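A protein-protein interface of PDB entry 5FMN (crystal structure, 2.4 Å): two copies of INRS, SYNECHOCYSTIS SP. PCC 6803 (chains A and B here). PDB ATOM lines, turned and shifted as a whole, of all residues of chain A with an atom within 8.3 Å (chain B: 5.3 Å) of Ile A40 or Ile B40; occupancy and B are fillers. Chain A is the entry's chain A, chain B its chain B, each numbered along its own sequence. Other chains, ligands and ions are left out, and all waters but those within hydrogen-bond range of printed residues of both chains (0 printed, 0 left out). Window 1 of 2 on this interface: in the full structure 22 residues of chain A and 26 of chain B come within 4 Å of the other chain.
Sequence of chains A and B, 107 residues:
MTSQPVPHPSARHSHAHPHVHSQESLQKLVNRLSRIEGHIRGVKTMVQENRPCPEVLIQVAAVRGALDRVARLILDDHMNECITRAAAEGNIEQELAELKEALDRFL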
ATOM      1  N   LEU A  29      21.876 -18.309  17.103  1.00  0.00           N
ATOM      2  CA  LEU A  29      20.842 -17.713  17.949  1.00  0.00           C
ATOM      3  C   LEU A  29      21.075 -17.883  19.437  1.00  0.00           C
ATOM      4  O   LEU A  29      20.809 -16.976  20.209  1.00  0.00           O
ATOM      5  CB  LEU A  29      19.479 -18.298  17.656  1.00  0.00           C
ATOM      6  CG  LEU A  29      18.804 -17.365  16.650  1.00  0.00           C
ATOM      7  CD1 LEU A  29      19.262 -17.639  15.220  1.00  0.00           C
ATOM      8  CD2 LEU A  29      17.299 -17.452  16.781  1.00  0.00           C
ATOM      9  N   VAL A  30      21.500 -19.071  19.832  1.00  0.00           N
ATOM     10  CA  VAL A  30      21.847 -19.332  21.217  1.00  0.00           C
ATOM     11  C   VAL A  30      22.918 -18.348  21.673  1.00  0.00           C
ATOM     12  O   VAL A  30      22.830 -17.773  22.767  1.00  0.00           O
ATOM     13  CB  VAL A  30      22.301 -20.810  21.416  1.00  0.00           C
ATOM     14  CG1 VAL A  30      23.023 -21.004  22.756  1.00  0.00           C
ATOM     15  CG2 VAL A  30      21.093 -21.734  21.292  1.00  0.00           C
ATOM     16  N   ARG A  32      23.617 -15.368  20.462  1.00  0.00           N
ATOM     17  CA  ARG A  32      23.108 -14.017  20.571  1.00  0.00           C
ATOM     18  C   ARG A  32      22.391 -13.864  21.876  1.00  0.00           C
ATOM     19  O   ARG A  32      22.518 -12.833  22.530  1.00  0.00           O
ATOM     20  CB  ARG A  32      22.153 -13.643  19.417  1.00  0.00           C
ATOM     21  CG  ARG A  32      22.852 -13.415  18.102  1.00  0.00           C
ATOM     22  CD  ARG A  32      21.863 -12.989  17.009  1.00  0.00           C
ATOM     23  NE  ARG A  32      22.551 -12.404  15.859  1.00  0.00           N
ATOM     24  CZ  ARG A  32      22.945 -11.135  15.782  1.00  0.00           C
ATOM     25  NH1 ARG A  32      22.674 -10.251  16.743  1.00  0.00           N
ATOM     26  NH2 ARG A  32      23.603 -10.738  14.710  1.00  0.00           N
ATOM     27  N   LEU A  33      21.636 -14.897  22.249  1.00  0.00           N
ATOM     28  CA  LEU A  33      20.875 -14.880  23.473  1.00  0.00           C
ATOM     29  C   LEU A  33      21.739 -14.941  24.736  1.00  0.00           C
ATOM     30  O   LEU A  33      21.464 -14.250  25.683  1.00  0.00           O
ATOM     31  CB  LEU A  33      19.892 -16.030  23.483  1.00  0.00           C
ATOM     32  CG  LEU A  33      18.707 -15.897  22.532  1.00  0.00           C
ATOM     33  CD1 LEU A  33      18.049 -17.247  22.286  1.00  0.00           C
ATOM     34  CD2 LEU A  33      17.714 -14.908  23.111  1.00  0.00           C
ATOM     35  N   SER A  34      22.807 -15.714  24.727  1.00  0.00           N
ATOM     36  CA  SER A  34      23.846 -15.612  25.764  1.00  0.00           C
ATOM     37  C   SER A  34      24.445 -14.208  25.898  1.00  0.00           C
ATOM     38  O   SER A  34      24.623 -13.747  27.016  1.00  0.00           O
ATOM     39  CB  SER A  34      24.980 -16.611  25.517  1.00  0.00           C
ATOM     40  OG  SER A  34      24.473 -17.912  25.582  1.00  0.00           O
ATOM     41  N   ARG A  35      24.720 -13.533  24.778  1.00  0.00           N
ATOM     42  CA  ARG A  35      25.256 -12.152  24.813  1.00  0.00           C
ATOM     43  C   ARG A  35      24.271 -11.176  25.396  1.00  0.00           C
ATOM     44  O   ARG A  35      24.642 -10.272  26.114  1.00  0.00           O
ATOM     45  CB  ARG A  35      25.627 -11.651  23.424  1.00  0.00           C
ATOM     46  CG  ARG A  35      27.011 -12.095  22.995  1.00  0.00           C
ATOM     47  CD  ARG A  35      27.523 -11.268  21.819  1.00  0.00           C
ATOM     48  NE  ARG A  35      27.350 -12.019  20.582  1.00  0.00           N
ATOM     49  CZ  ARG A  35      26.542 -11.667  19.578  1.00  0.00           C
ATOM     50  NH1 ARG A  35      25.825 -10.529  19.623  1.00  0.00           N
ATOM     51  NH2 ARG A  35      26.466 -12.459  18.505  1.00  0.00           N
ATOM     52  N   ILE A  36      23.008 -11.333  25.053  1.00  0.00           N
ATOM     53  CA  ILE A  36      21.964 -10.505  25.634  1.00  0.00           C
ATOM     54  C   ILE A  36      21.890 -10.700  27.167  1.00  0.00           C
ATOM     55  O   ILE A  36      21.714  -9.747  27.908  1.00  0.00           O
ATOM     56  CB  ILE A  36      20.607 -10.818  24.969  1.00  0.00           C
ATOM     57  CG1 ILE A  36      20.571 -10.229  23.558  1.00  0.00           C
ATOM     58  CG2 ILE A  36      19.435 -10.301  25.797  1.00  0.00           C
ATOM     59  CD1 ILE A  36      19.383 -10.741  22.756  1.00  0.00           C
ATOM     60  N   GLU A  37      21.983 -11.945  27.612  1.00  0.00           N
ATOM     61  CA  GLU A  37      22.000 -12.312  29.039  1.00  0.00           C
ATOM     62  C   GLU A  37      23.161 -11.650  29.780  1.00  0.00           C
ATOM     63  O   GLU A  37      22.972 -10.995  30.821  1.00  0.00           O
ATOM     64  CB  GLU A  37      22.118 -13.839  29.115  1.00  0.00           C
ATOM     65  CG  GLU A  37      21.503 -14.543  30.303  1.00  0.00           C
ATOM     66  CD  GLU A  37      21.985 -15.981  30.411  1.00  0.00           C
ATOM     67  OE1 GLU A  37      22.141 -16.653  29.364  1.00  0.00           O
ATOM     68  OE2 GLU A  37      22.205 -16.444  31.549  1.00  0.00           O
ATOM     69  N   GLY A  38      24.350 -11.734  29.193  1.00  0.00           N
ATOM     70  CA  GLY A  38      25.542 -11.012  29.712  1.00  0.00           C
ATOM     71  C   GLY A  38      25.384  -9.482  29.767  1.00  0.00           C
ATOM     72  O   GLY A  38      25.887  -8.793  30.653  1.00  0.00           O
ATOM     73  N   HIS A  39      24.674  -8.951  28.801  1.00  0.00           N
ATOM     74  CA  HIS A  39      24.423  -7.541  28.724  1.00  0.00           C
ATOM     75  C   HIS A  39      23.442  -7.081  29.771  1.00  0.00           C
ATOM     76  O   HIS A  39      23.500  -5.945  30.207  1.00  0.00           O
ATOM     77  CB  HIS A  39      23.815  -7.229  27.368  1.00  0.00           C
ATOM     78  CG  HIS A  39      24.317  -5.981  26.784  1.00  0.00           C
ATOM     79  ND1 HIS A  39      24.686  -5.883  25.466  1.00  0.00           N
ATOM     80  CD2 HIS A  39      24.487  -4.756  27.336  1.00  0.00           C
ATOM     81  CE1 HIS A  39      25.065  -4.639  25.229  1.00  0.00           C
ATOM     82  NE2 HIS A  39      24.931  -3.931  26.340  1.00  0.00           N
ATOM     83  N   ILE A  40      22.474  -7.925  30.105  1.00  0.00           N
ATOM     84  CA  ILE A  40      21.548  -7.600  31.182  1.00  0.00           C
ATOM     85  C   ILE A  40      22.237  -7.656  32.529  1.00  0.00           C
ATOM     86  O   ILE A  40      21.957  -6.818  33.360  1.00  0.00           O
ATOM     87  CB  ILE A  40      20.298  -8.505  31.169  1.00  0.00           C
ATOM     88  CG1 ILE A  40      19.228  -7.835  30.337  1.00  0.00           C
ATOM     89  CG2 ILE A  40      19.713  -8.711  32.564  1.00  0.00           C
ATOM     90  CD1 ILE A  40      18.428  -8.850  29.584  1.00  0.00           C
ATOM     91  N   ARG A  41      23.161  -8.604  32.716  1.00  0.00           N
ATOM     92  CA  ARG A  41      24.010  -8.585  33.920  1.00  0.00           C
ATOM     93  C   ARG A  41      24.760  -7.244  34.016  1.00  0.00           C
ATOM     94  O   ARG A  41      24.912  -6.694  35.105  1.00  0.00           O
ATOM     95  CB  ARG A  41      25.019  -9.746  34.031  1.00  0.00           C
ATOM     96  CG  ARG A  41      24.473 -11.167  33.948  1.00  0.00           C
ATOM     97  CD  ARG A  41      25.529 -12.226  34.288  1.00  0.00           C
ATOM     98  NE  ARG A  41      26.503 -12.474  33.235  1.00  0.00           N
ATOM     99  CZ  ARG A  41      26.430 -13.437  32.297  1.00  0.00           C
ATOM    100  NH1 ARG A  41      25.426 -14.325  32.240  1.00  0.00           N
ATOM    101  NH2 ARG A  41      27.405 -13.516  31.400  1.00  0.00           N
ATOM    102  N   GLY A  42      25.256  -6.758  32.886  1.00  0.00           N
ATOM    103  CA  GLY A  42      26.000  -5.502  32.832  1.00  0.00           C
ATOM    104  C   GLY A  42      25.176  -4.318  33.287  1.00  0.00           C
ATOM    105  O   GLY A  42      25.629  -3.528  34.079  1.00  0.00           O
ATOM    106  N   VAL A  43      23.937  -4.239  32.833  1.00  0.00           N
ATOM    107  CA  VAL A  43      22.979  -3.263  33.342  1.00  0.00           C
ATOM    108  C   VAL A  43      22.733  -3.377  34.853  1.00  0.00           C
ATOM    109  O   VAL A  43      22.590  -2.343  35.514  1.00  0.00           O
ATOM    110  CB  VAL A  43      21.619  -3.382  32.622  1.00  0.00           C
ATOM    111  CG1 VAL A  43      20.613  -2.376  33.158  1.00  0.00           C
ATOM    112  CG2 VAL A  43      21.812  -3.160  31.129  1.00  0.00           C
ATOM    113  N   LYS A  44      22.711  -4.611  35.388  1.00  0.00           N
ATOM    114  CA  LYS A  44      22.523  -4.841  36.826  1.00  0.00           C
ATOM    115  C   LYS A  44      23.688  -4.285  37.644  1.00  0.00           C
ATOM    116  O   LYS A  44      23.480  -3.565  38.625  1.00  0.00           O
ATOM    117  CB  LYS A  44      22.332  -6.335  37.123  1.00  0.00           C
ATOM    118  CG  LYS A  44      22.281  -6.707  38.606  1.00  0.00           C
ATOM    119  CD  LYS A  44      21.907  -8.158  38.795  1.00  0.00           C
ATOM    120  CE  LYS A  44      22.788  -9.079  37.976  1.00  0.00           C
ATOM    121  NZ  LYS A  44      24.180  -8.663  38.189  1.00  0.00           N
ATOM    122  N   THR A  45      24.898  -4.656  37.263  1.00  0.00           N
ATOM    123  CA  THR A  45      26.098  -4.083  37.837  1.00  0.00           C
ATOM    124  C   THR A  45      26.069  -2.565  37.830  1.00  0.00           C
ATOM    125  O   THR A  45      26.403  -1.945  38.830  1.00  0.00           O
ATOM    126  CB  THR A  45      27.325  -4.587  37.078  1.00  0.00           C
ATOM    127  OG1 THR A  45      27.480  -5.984  37.349  1.00  0.00           O
ATOM    128  CG2 THR A  45      28.569  -3.845  37.509  1.00  0.00           C
ATOM    129  N   MET A  46      25.631  -1.963  36.731  1.00  0.00           N
ATOM    130  CA  MET A  46      25.621  -0.496  36.629  1.00  0.00           C
ATOM    131  C   MET A  46      24.696   0.136  37.671  1.00  0.00           C
ATOM    132  O   MET A  46      24.936   1.224  38.146  1.00  0.00           O
ATOM    133  CB  MET A  46      25.166  -0.033  35.242  1.00  0.00           C
ATOM    134  CG  MET A  46      26.214  -0.171  34.148  1.00  0.00           C
ATOM    135  SD  MET A  46      25.684   0.493  32.545  1.00  0.00           S
ATOM    136  CE  MET A  46      25.466   2.211  32.924  1.00  0.00           C
ATOM    137  N   VAL A  47      23.584  -0.509  37.918  1.00  0.00           N
ATOM    138  CA  VAL A  47      22.609  -0.002  38.847  1.00  0.00           C
ATOM    139  C   VAL A  47      23.164  -0.087  40.285  1.00  0.00           C
ATOM    140  O   VAL A  47      23.039   0.878  41.042  1.00  0.00           O
ATOM    141  CB  VAL A  47      21.281  -0.787  38.715  1.00  0.00           C
ATOM    142  CG1 VAL A  47      20.341  -0.484  39.873  1.00  0.00           C
ATOM    143  CG2 VAL A  47      20.612  -0.456  37.397  1.00  0.00           C
ATOM    144  N   GLN A  59      22.573   1.667  27.879  1.00  0.00           N
ATOM    145  CA  GLN A  59      22.822   0.222  27.931  1.00  0.00           C
ATOM    146  C   GLN A  59      21.522  -0.631  27.772  1.00  0.00           C
ATOM    147  O   GLN A  59      21.485  -1.624  27.043  1.00  0.00           O
ATOM    148  CB  GLN A  59      23.567  -0.093  29.252  1.00  0.00           C
ATOM    149  CG  GLN A  59      24.701  -1.094  29.118  1.00  0.00           C
ATOM    150  CD  GLN A  59      25.759  -0.675  28.083  1.00  0.00           C
ATOM    151  OE1 GLN A  59      25.849  -1.346  27.086  1.00  0.00           O
ATOM    152  NE2 GLN A  59      26.508   0.462  28.274  1.00  0.00           N
ATOM    153  N   VAL A  60      20.449  -0.193  28.408  1.00  0.00           N
ATOM    154  CA  VAL A  60      19.103  -0.782  28.232  1.00  0.00           C
ATOM    155  C   VAL A  60      18.619  -0.686  26.777  1.00  0.00           C
ATOM    156  O   VAL A  60      18.016  -1.633  26.288  1.00  0.00           O
ATOM    157  CB  VAL A  60      18.073  -0.045  29.136  1.00  0.00           C
ATOM    158  CG1 VAL A  60      16.646  -0.478  28.843  1.00  0.00           C
ATOM    159  CG2 VAL A  60      18.386  -0.258  30.627  1.00  0.00           C
ATOM    160  N   VAL A  63      20.399  -3.325  24.775  1.00  0.00           N
ATOM    161  CA  VAL A  63      19.798  -4.630  25.079  1.00  0.00           C
ATOM    162  C   VAL A  63      18.476  -4.761  24.305  1.00  0.00           C
ATOM    163  O   VAL A  63      18.170  -5.812  23.716  1.00  0.00           O
ATOM    164  CB  VAL A  63      19.486  -4.786  26.587  1.00  0.00           C
ATOM    165  CG1 VAL A  63      18.684  -6.040  26.860  1.00  0.00           C
ATOM    166  CG2 VAL A  63      20.750  -4.797  27.413  1.00  0.00           C
ATOM    167  N   ARG A  64      17.687  -3.698  24.298  1.00  0.00           N
ATOM    168  CA  ARG A  64      16.427  -3.754  23.559  1.00  0.00           C
ATOM    169  C   ARG A  64      16.652  -3.905  22.056  1.00  0.00           C
ATOM    170  O   ARG A  64      16.020  -4.715  21.397  1.00  0.00           O
ATOM    171  CB  ARG A  64      15.590  -2.551  23.872  1.00  0.00           C
ATOM    172  CG  ARG A  64      14.455  -2.367  22.907  1.00  0.00           C
ATOM    173  CD  ARG A  64      13.370  -1.547  23.587  1.00  0.00           C
ATOM    174  NE  ARG A  64      13.959  -0.316  24.114  1.00  0.00           N
ATOM    175  CZ  ARG A  64      13.931   0.084  25.387  1.00  0.00           C
ATOM    176  NH1 ARG A  64      13.262  -0.595  26.314  1.00  0.00           N
ATOM    177  NH2 ARG A  64      14.580   1.193  25.730  1.00  0.00           N
ATOM    178  N   LEU A  67      17.575  -7.508  21.399  1.00  0.00           N
ATOM    179  CA  LEU A  67      16.392  -8.348  21.498  1.00  0.00           C
ATOM    180  C   LEU A  67      15.526  -8.260  20.235  1.00  0.00           C
ATOM    181  O   LEU A  67      15.071  -9.263  19.722  1.00  0.00           O
ATOM    182  CB  LEU A  67      15.580  -7.897  22.692  1.00  0.00           C
ATOM    183  CG  LEU A  67      14.441  -8.804  23.095  1.00  0.00           C
ATOM    184  CD1 LEU A  67      15.010 -10.136  23.538  1.00  0.00           C
ATOM    185  CD2 LEU A  67      13.692  -8.113  24.207  1.00  0.00           C
ATOM    186  N   LEU B  33      15.671  -7.083  37.249  1.00  0.00           N
ATOM    187  CA  LEU B  33      16.686  -7.413  36.256  1.00  0.00           C
ATOM    188  C   LEU B  33      17.140  -8.871  36.308  1.00  0.00           C
ATOM    189  O   LEU B  33      17.484  -9.442  35.278  1.00  0.00           O
ATOM    190  CB  LEU B  33      17.887  -6.466  36.401  1.00  0.00           C
ATOM    191  CG  LEU B  33      17.605  -5.016  35.976  1.00  0.00           C
ATOM    192  CD1 LEU B  33      18.649  -4.072  36.541  1.00  0.00           C
ATOM    193  CD2 LEU B  33      17.579  -4.929  34.458  1.00  0.00           C
ATOM    194  N   ARG B  35      15.175 -11.305  37.211  1.00  0.00           N
ATOM    195  CA  ARG B  35      14.040 -11.996  36.572  1.00  0.00           C
ATOM    196  C   ARG B  35      14.130 -11.956  35.060  1.00  0.00           C
ATOM    197  O   ARG B  35      13.818 -12.927  34.382  1.00  0.00           O
ATOM    198  CB  ARG B  35      12.688 -11.393  36.991  1.00  0.00           C
ATOM    199  CG  ARG B  35      12.127 -11.886  38.321  1.00  0.00           C
ATOM    200  CD  ARG B  35      10.734 -11.337  38.551  1.00  0.00           C
ATOM    201  NE  ARG B  35       9.754 -12.319  39.039  1.00  0.00           N
ATOM    202  CZ  ARG B  35       8.643 -12.669  38.376  1.00  0.00           C
ATOM    203  NH1 ARG B  35       8.368 -12.116  37.194  1.00  0.00           N
ATOM    204  NH2 ARG B  35       7.811 -13.581  38.890  1.00  0.00           N
ATOM    205  N   ILE B  36      14.542 -10.824  34.522  1.00  0.00           N
ATOM    206  CA  ILE B  36      14.688 -10.672  33.060  1.00  0.00           C
ATOM    207  C   ILE B  36      15.812 -11.544  32.496  1.00  0.00           C
ATOM    208  O   ILE B  36      15.642 -12.210  31.467  1.00  0.00           O
ATOM    209  CB  ILE B  36      14.955  -9.208  32.744  1.00  0.00           C
ATOM    210  CG1 ILE B  36      13.666  -8.434  32.915  1.00  0.00           C
ATOM    211  CG2 ILE B  36      15.551  -9.042  31.372  1.00  0.00           C
ATOM    212  CD1 ILE B  36      13.882  -6.933  32.921  1.00  0.00           C
ATOM    213  N   GLU B  37      16.921 -11.598  33.227  1.00  0.00           N
ATOM    214  CA  GLU B  37      18.017 -12.537  32.954  1.00  0.00           C
ATOM    215  C   GLU B  37      17.567 -14.008  32.898  1.00  0.00           C
ATOM    216  O   GLU B  37      17.899 -14.743  31.959  1.00  0.00           O
ATOM    217  CB  GLU B  37      19.090 -12.378  34.049  1.00  0.00           C
ATOM    218  CG  GLU B  37      20.472 -12.810  33.625  1.00  0.00           C
ATOM    219  CD  GLU B  37      21.377 -13.053  34.807  1.00  0.00           C
ATOM    220  OE1 GLU B  37      21.318 -12.245  35.767  1.00  0.00           O
ATOM    221  OE2 GLU B  37      22.151 -14.046  34.753  1.00  0.00           O
ATOM    222  N   GLY B  38      16.833 -14.435  33.932  1.00  0.00           N
ATOM    223  CA  GLY B  38      16.266 -15.795  33.990  1.00  0.00           C
ATOM    224  C   GLY B  38      15.315 -16.086  32.840  1.00  0.00           C
ATOM    225  O   GLY B  38      15.240 -17.191  32.343  1.00  0.00           O
ATOM    226  N   HIS B  39      14.613 -15.063  32.405  1.00  0.00           N
ATOM    227  CA  HIS B  39      13.666 -15.174  31.323  1.00  0.00           C
ATOM    228  C   HIS B  39      14.347 -15.283  29.973  1.00  0.00           C
ATOM    229  O   HIS B  39      13.853 -15.966  29.081  1.00  0.00           O
ATOM    230  CB  HIS B  39      12.808 -13.935  31.319  1.00  0.00           C
ATOM    231  CG  HIS B  39      11.375 -14.195  31.604  1.00  0.00           C
ATOM    232  ND1 HIS B  39      10.461 -14.495  30.617  1.00  0.00           N
ATOM    233  CD2 HIS B  39      10.694 -14.175  32.776  1.00  0.00           C
ATOM    234  CE1 HIS B  39       9.273 -14.649  31.173  1.00  0.00           C
ATOM    235  NE2 HIS B  39       9.391 -14.475  32.480  1.00  0.00           N
ATOM    236  N   ILE B  40      15.477 -14.605  29.820  1.00  0.00           N
ATOM    237  CA  ILE B  40      16.286 -14.776  28.609  1.00  0.00           C
ATOM    238  C   ILE B  40      16.937 -16.138  28.531  1.00  0.00           C
ATOM    239  O   ILE B  40      17.022 -16.728  27.455  1.00  0.00           O
ATOM    240  CB  ILE B  40      17.353 -13.683  28.482  1.00  0.00           C
ATOM    241  CG1 ILE B  40      16.753 -12.538  27.718  1.00  0.00           C
ATOM    242  CG2 ILE B  40      18.576 -14.140  27.712  1.00  0.00           C
ATOM    243  CD1 ILE B  40      17.267 -11.228  28.232  1.00  0.00           C
ATOM    244  N   ARG B  41      17.396 -16.639  29.664  1.00  0.00           N
ATOM    245  CA  ARG B  41      17.943 -17.990  29.722  1.00  0.00           C
ATOM    246  C   ARG B  41      16.851 -19.030  29.353  1.00  0.00           C
ATOM    247  O   ARG B  41      17.098 -19.974  28.580  1.00  0.00           O
ATOM    248  CB  ARG B  41      18.509 -18.177  31.131  1.00  0.00           C
ATOM    249  CG  ARG B  41      19.648 -19.130  31.227  1.00  0.00           C
ATOM    250  CD  ARG B  41      20.149 -19.169  32.647  1.00  0.00           C
ATOM    251  NE  ARG B  41      21.120 -20.240  32.794  1.00  0.00           N
ATOM    252  CZ  ARG B  41      22.400 -20.148  32.469  1.00  0.00           C
ATOM    253  NH1 ARG B  41      22.903 -19.002  31.998  1.00  0.00           N
ATOM    254  NH2 ARG B  41      23.195 -21.197  32.659  1.00  0.00           N
ATOM    255  N   GLY B  42      15.611 -18.770  29.772  1.00  0.00           N
ATOM    256  CA  GLY B  42      14.456 -19.564  29.346  1.00  0.00           C
ATOM    257  C   GLY B  42      14.200 -19.598  27.848  1.00  0.00           C
ATOM    258  O   GLY B  42      13.917 -20.647  27.288  1.00  0.00           O
ATOM    259  N   VAL B  43      14.283 -18.447  27.195  1.00  0.00           N
ATOM    260  CA  VAL B  43      14.203 -18.382  25.729  1.00  0.00           C
ATOM    261  C   VAL B  43      15.297 -19.230  25.070  1.00  0.00           C
ATOM    262  O   VAL B  43      15.062 -19.831  24.017  1.00  0.00           O
ATOM    263  CB  VAL B  43      14.301 -16.927  25.228  1.00  0.00           C
ATOM    264  CG1 VAL B  43      14.317 -16.845  23.700  1.00  0.00           C
ATOM    265  CG2 VAL B  43      13.146 -16.096  25.766  1.00  0.00           C
ATOM    266  N   LYS B  44      16.477 -19.269  25.684  1.00  0.00           N
ATOM    267  CA  LYS B  44      17.619 -20.008  25.123  1.00  0.00           C
ATOM    268  C   LYS B  44      17.370 -21.514  25.164  1.00  0.00           C
ATOM    269  O   LYS B  44      17.521 -22.204  24.156  1.00  0.00           O
ATOM    270  CB  LYS B  44      18.911 -19.633  25.835  1.00  0.00           C
ATOM    271  CG  LYS B  44      20.108 -20.434  25.375  1.00  0.00           C
ATOM    272  CD  LYS B  44      21.434 -19.778  25.760  1.00  0.00           C
ATOM    273  CE  LYS B  44      21.418 -19.253  27.186  1.00  0.00           C
ATOM    274  NZ  LYS B  44      22.734 -19.360  27.846  1.00  0.00           N
ATOM    275  N   VAL B  63       9.808 -10.801  27.526  1.00  0.00           N
ATOM    276  CA  VAL B  63      11.086 -10.268  27.963  1.00  0.00           C
ATOM    277  C   VAL B  63      11.217  -8.770  27.592  1.00  0.00           C
ATOM    278  O   VAL B  63      11.621  -7.943  28.398  1.00  0.00           O
ATOM    279  CB  VAL B  63      12.249 -11.015  27.279  1.00  0.00           C
ATOM    280  CG1 VAL B  63      13.562 -10.319  27.584  1.00  0.00           C
ATOM    281  CG2 VAL B  63      12.296 -12.463  27.710  1.00  0.00           C
ATOM    282  N   LEU B  67      11.520  -5.618  30.130  1.00  0.00           N
ATOM    283  CA  LEU B  67      12.574  -4.625  29.979  1.00  0.00           C
ATOM    284  C   LEU B  67      12.017  -3.206  29.944  1.00  0.00           C
ATOM    285  O   LEU B  67      12.575  -2.311  30.561  1.00  0.00           O
ATOM    286  CB  LEU B  67      13.374  -4.919  28.719  1.00  0.00           C
ATOM    287  CG  LEU B  67      14.683  -4.166  28.512  1.00  0.00           C
ATOM    288  CD1 LEU B  67      15.676  -4.450  29.633  1.00  0.00           C
ATOM    289  CD2 LEU B  67      15.275  -4.542  27.164  1.00  0.00           C
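The side-chain hydroxyl (OG) of Ser A34 sits at hydrogen-bond distance from the side-chain amino group (NZ) of Lys B44 (3.2 Å). The side-chain carboxylate (OE2) of Glu A37 is in salt-bridge range of the guanidinium group (NH1) of Arg B41 (2.7 Å). The side-chain carboxylate (OE1) of Glu A37 lies within salt-bridge range of the side-chain amino group (NZ) of Lys B44 (3.2 Å).
OG of Ser A34 is in hydrogen-bond range of O of Val A30. The side-chain carboxylate of Glu A37 lies within salt-bridge range of the guanidinium group of Arg A41, 3.9 Å away. O of Arg A41 lies within hydrogen-bond range of OG1 of Thr A45 (3.5 Å).
Among the printed residues, merely in contact across the chains: Ile A40 with Ile B40, Ile A36 with Ile B40, Ile A40 with Ile B36, Leu A33 with Ile B40, Ile A40 with Leu B33, Val A30 with Lys B44, Arg A41 with Glu B37, Val A63 with Leu B67, Glu A37 with Ile B40, Arg A64 with Leu B67, Glu A37 with Glu B37, Leu A33 with Val B43, Lys A44 with Leu B33 and Leu A33 with Lys B44.
Of the printed residues of chain B, Ile A40 touches Leu B33, Ile B36 and Ile B40. Of chain A, only Leu A33, Ile A36, Glu A37 and Ile A40 come within 4 Å of Ile B40. Of the printed residues of chain A, Glu B37 touches Glu A37 (3.9 Å) and Arg A41 (3.7 Å). Of the printed residues of chain B, Ile A36 touches Ile B40 (3.4 Å). Of the printed residues of chain A, Leu B67 touches Val A63 (3.7 Å) and Arg A64 (3.8 Å). Printed residues of chain A within 4 Å of Ile B36: Ile A40 (3.4 Å). Val B63 touches none of the printed residues of chain A. Arg A32 touches none of the printed residues of chain B. The nearest printed residue of chain B that does not touch Ile A40 is Glu B37 (4.01 Å). The nearest printed residue of chain A that does not touch Ile B40 is Leu A67 (5.1 Å).
Of the 23 printed residues of chain A, 10 touch a printed residue of chain B. Printed residues of chain A that touch a printed residue of chain B: Val A30, Leu A33, Ser A34, Ile A36, Glu A37, Ile A40, Arg A41, Lys A44, Val A63 and Arg A64. Hydrophobic or aromatic side chains of chain A within 4 Å of the printed part of chain B: Val A30, Leu A33, Ile A36, Ile A40 and Val A63. Of the 13 printed residues of chain B, 8 touch a printed residue of chain A. Printed residues of chain B that touch a printed residue of chain A: Leu B33, Ile B36, Glu B37, Ile B40, Arg B41, Val B43, Lys B44 and Leu B67. Among the printed residues, 17 pairs touch across the chains.
Leu A33 touches Ile B40, and with the chains exchanged Ile A40 touches Leu B33. Ile A36 touches Ile B40, and with the chains exchanged Ile A40 touches Ile B36. Glu A37 touches Arg B41, and with the chains exchanged Arg A41 touches Glu B37. Ile B40 touches its own counterpart, Ile A40.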
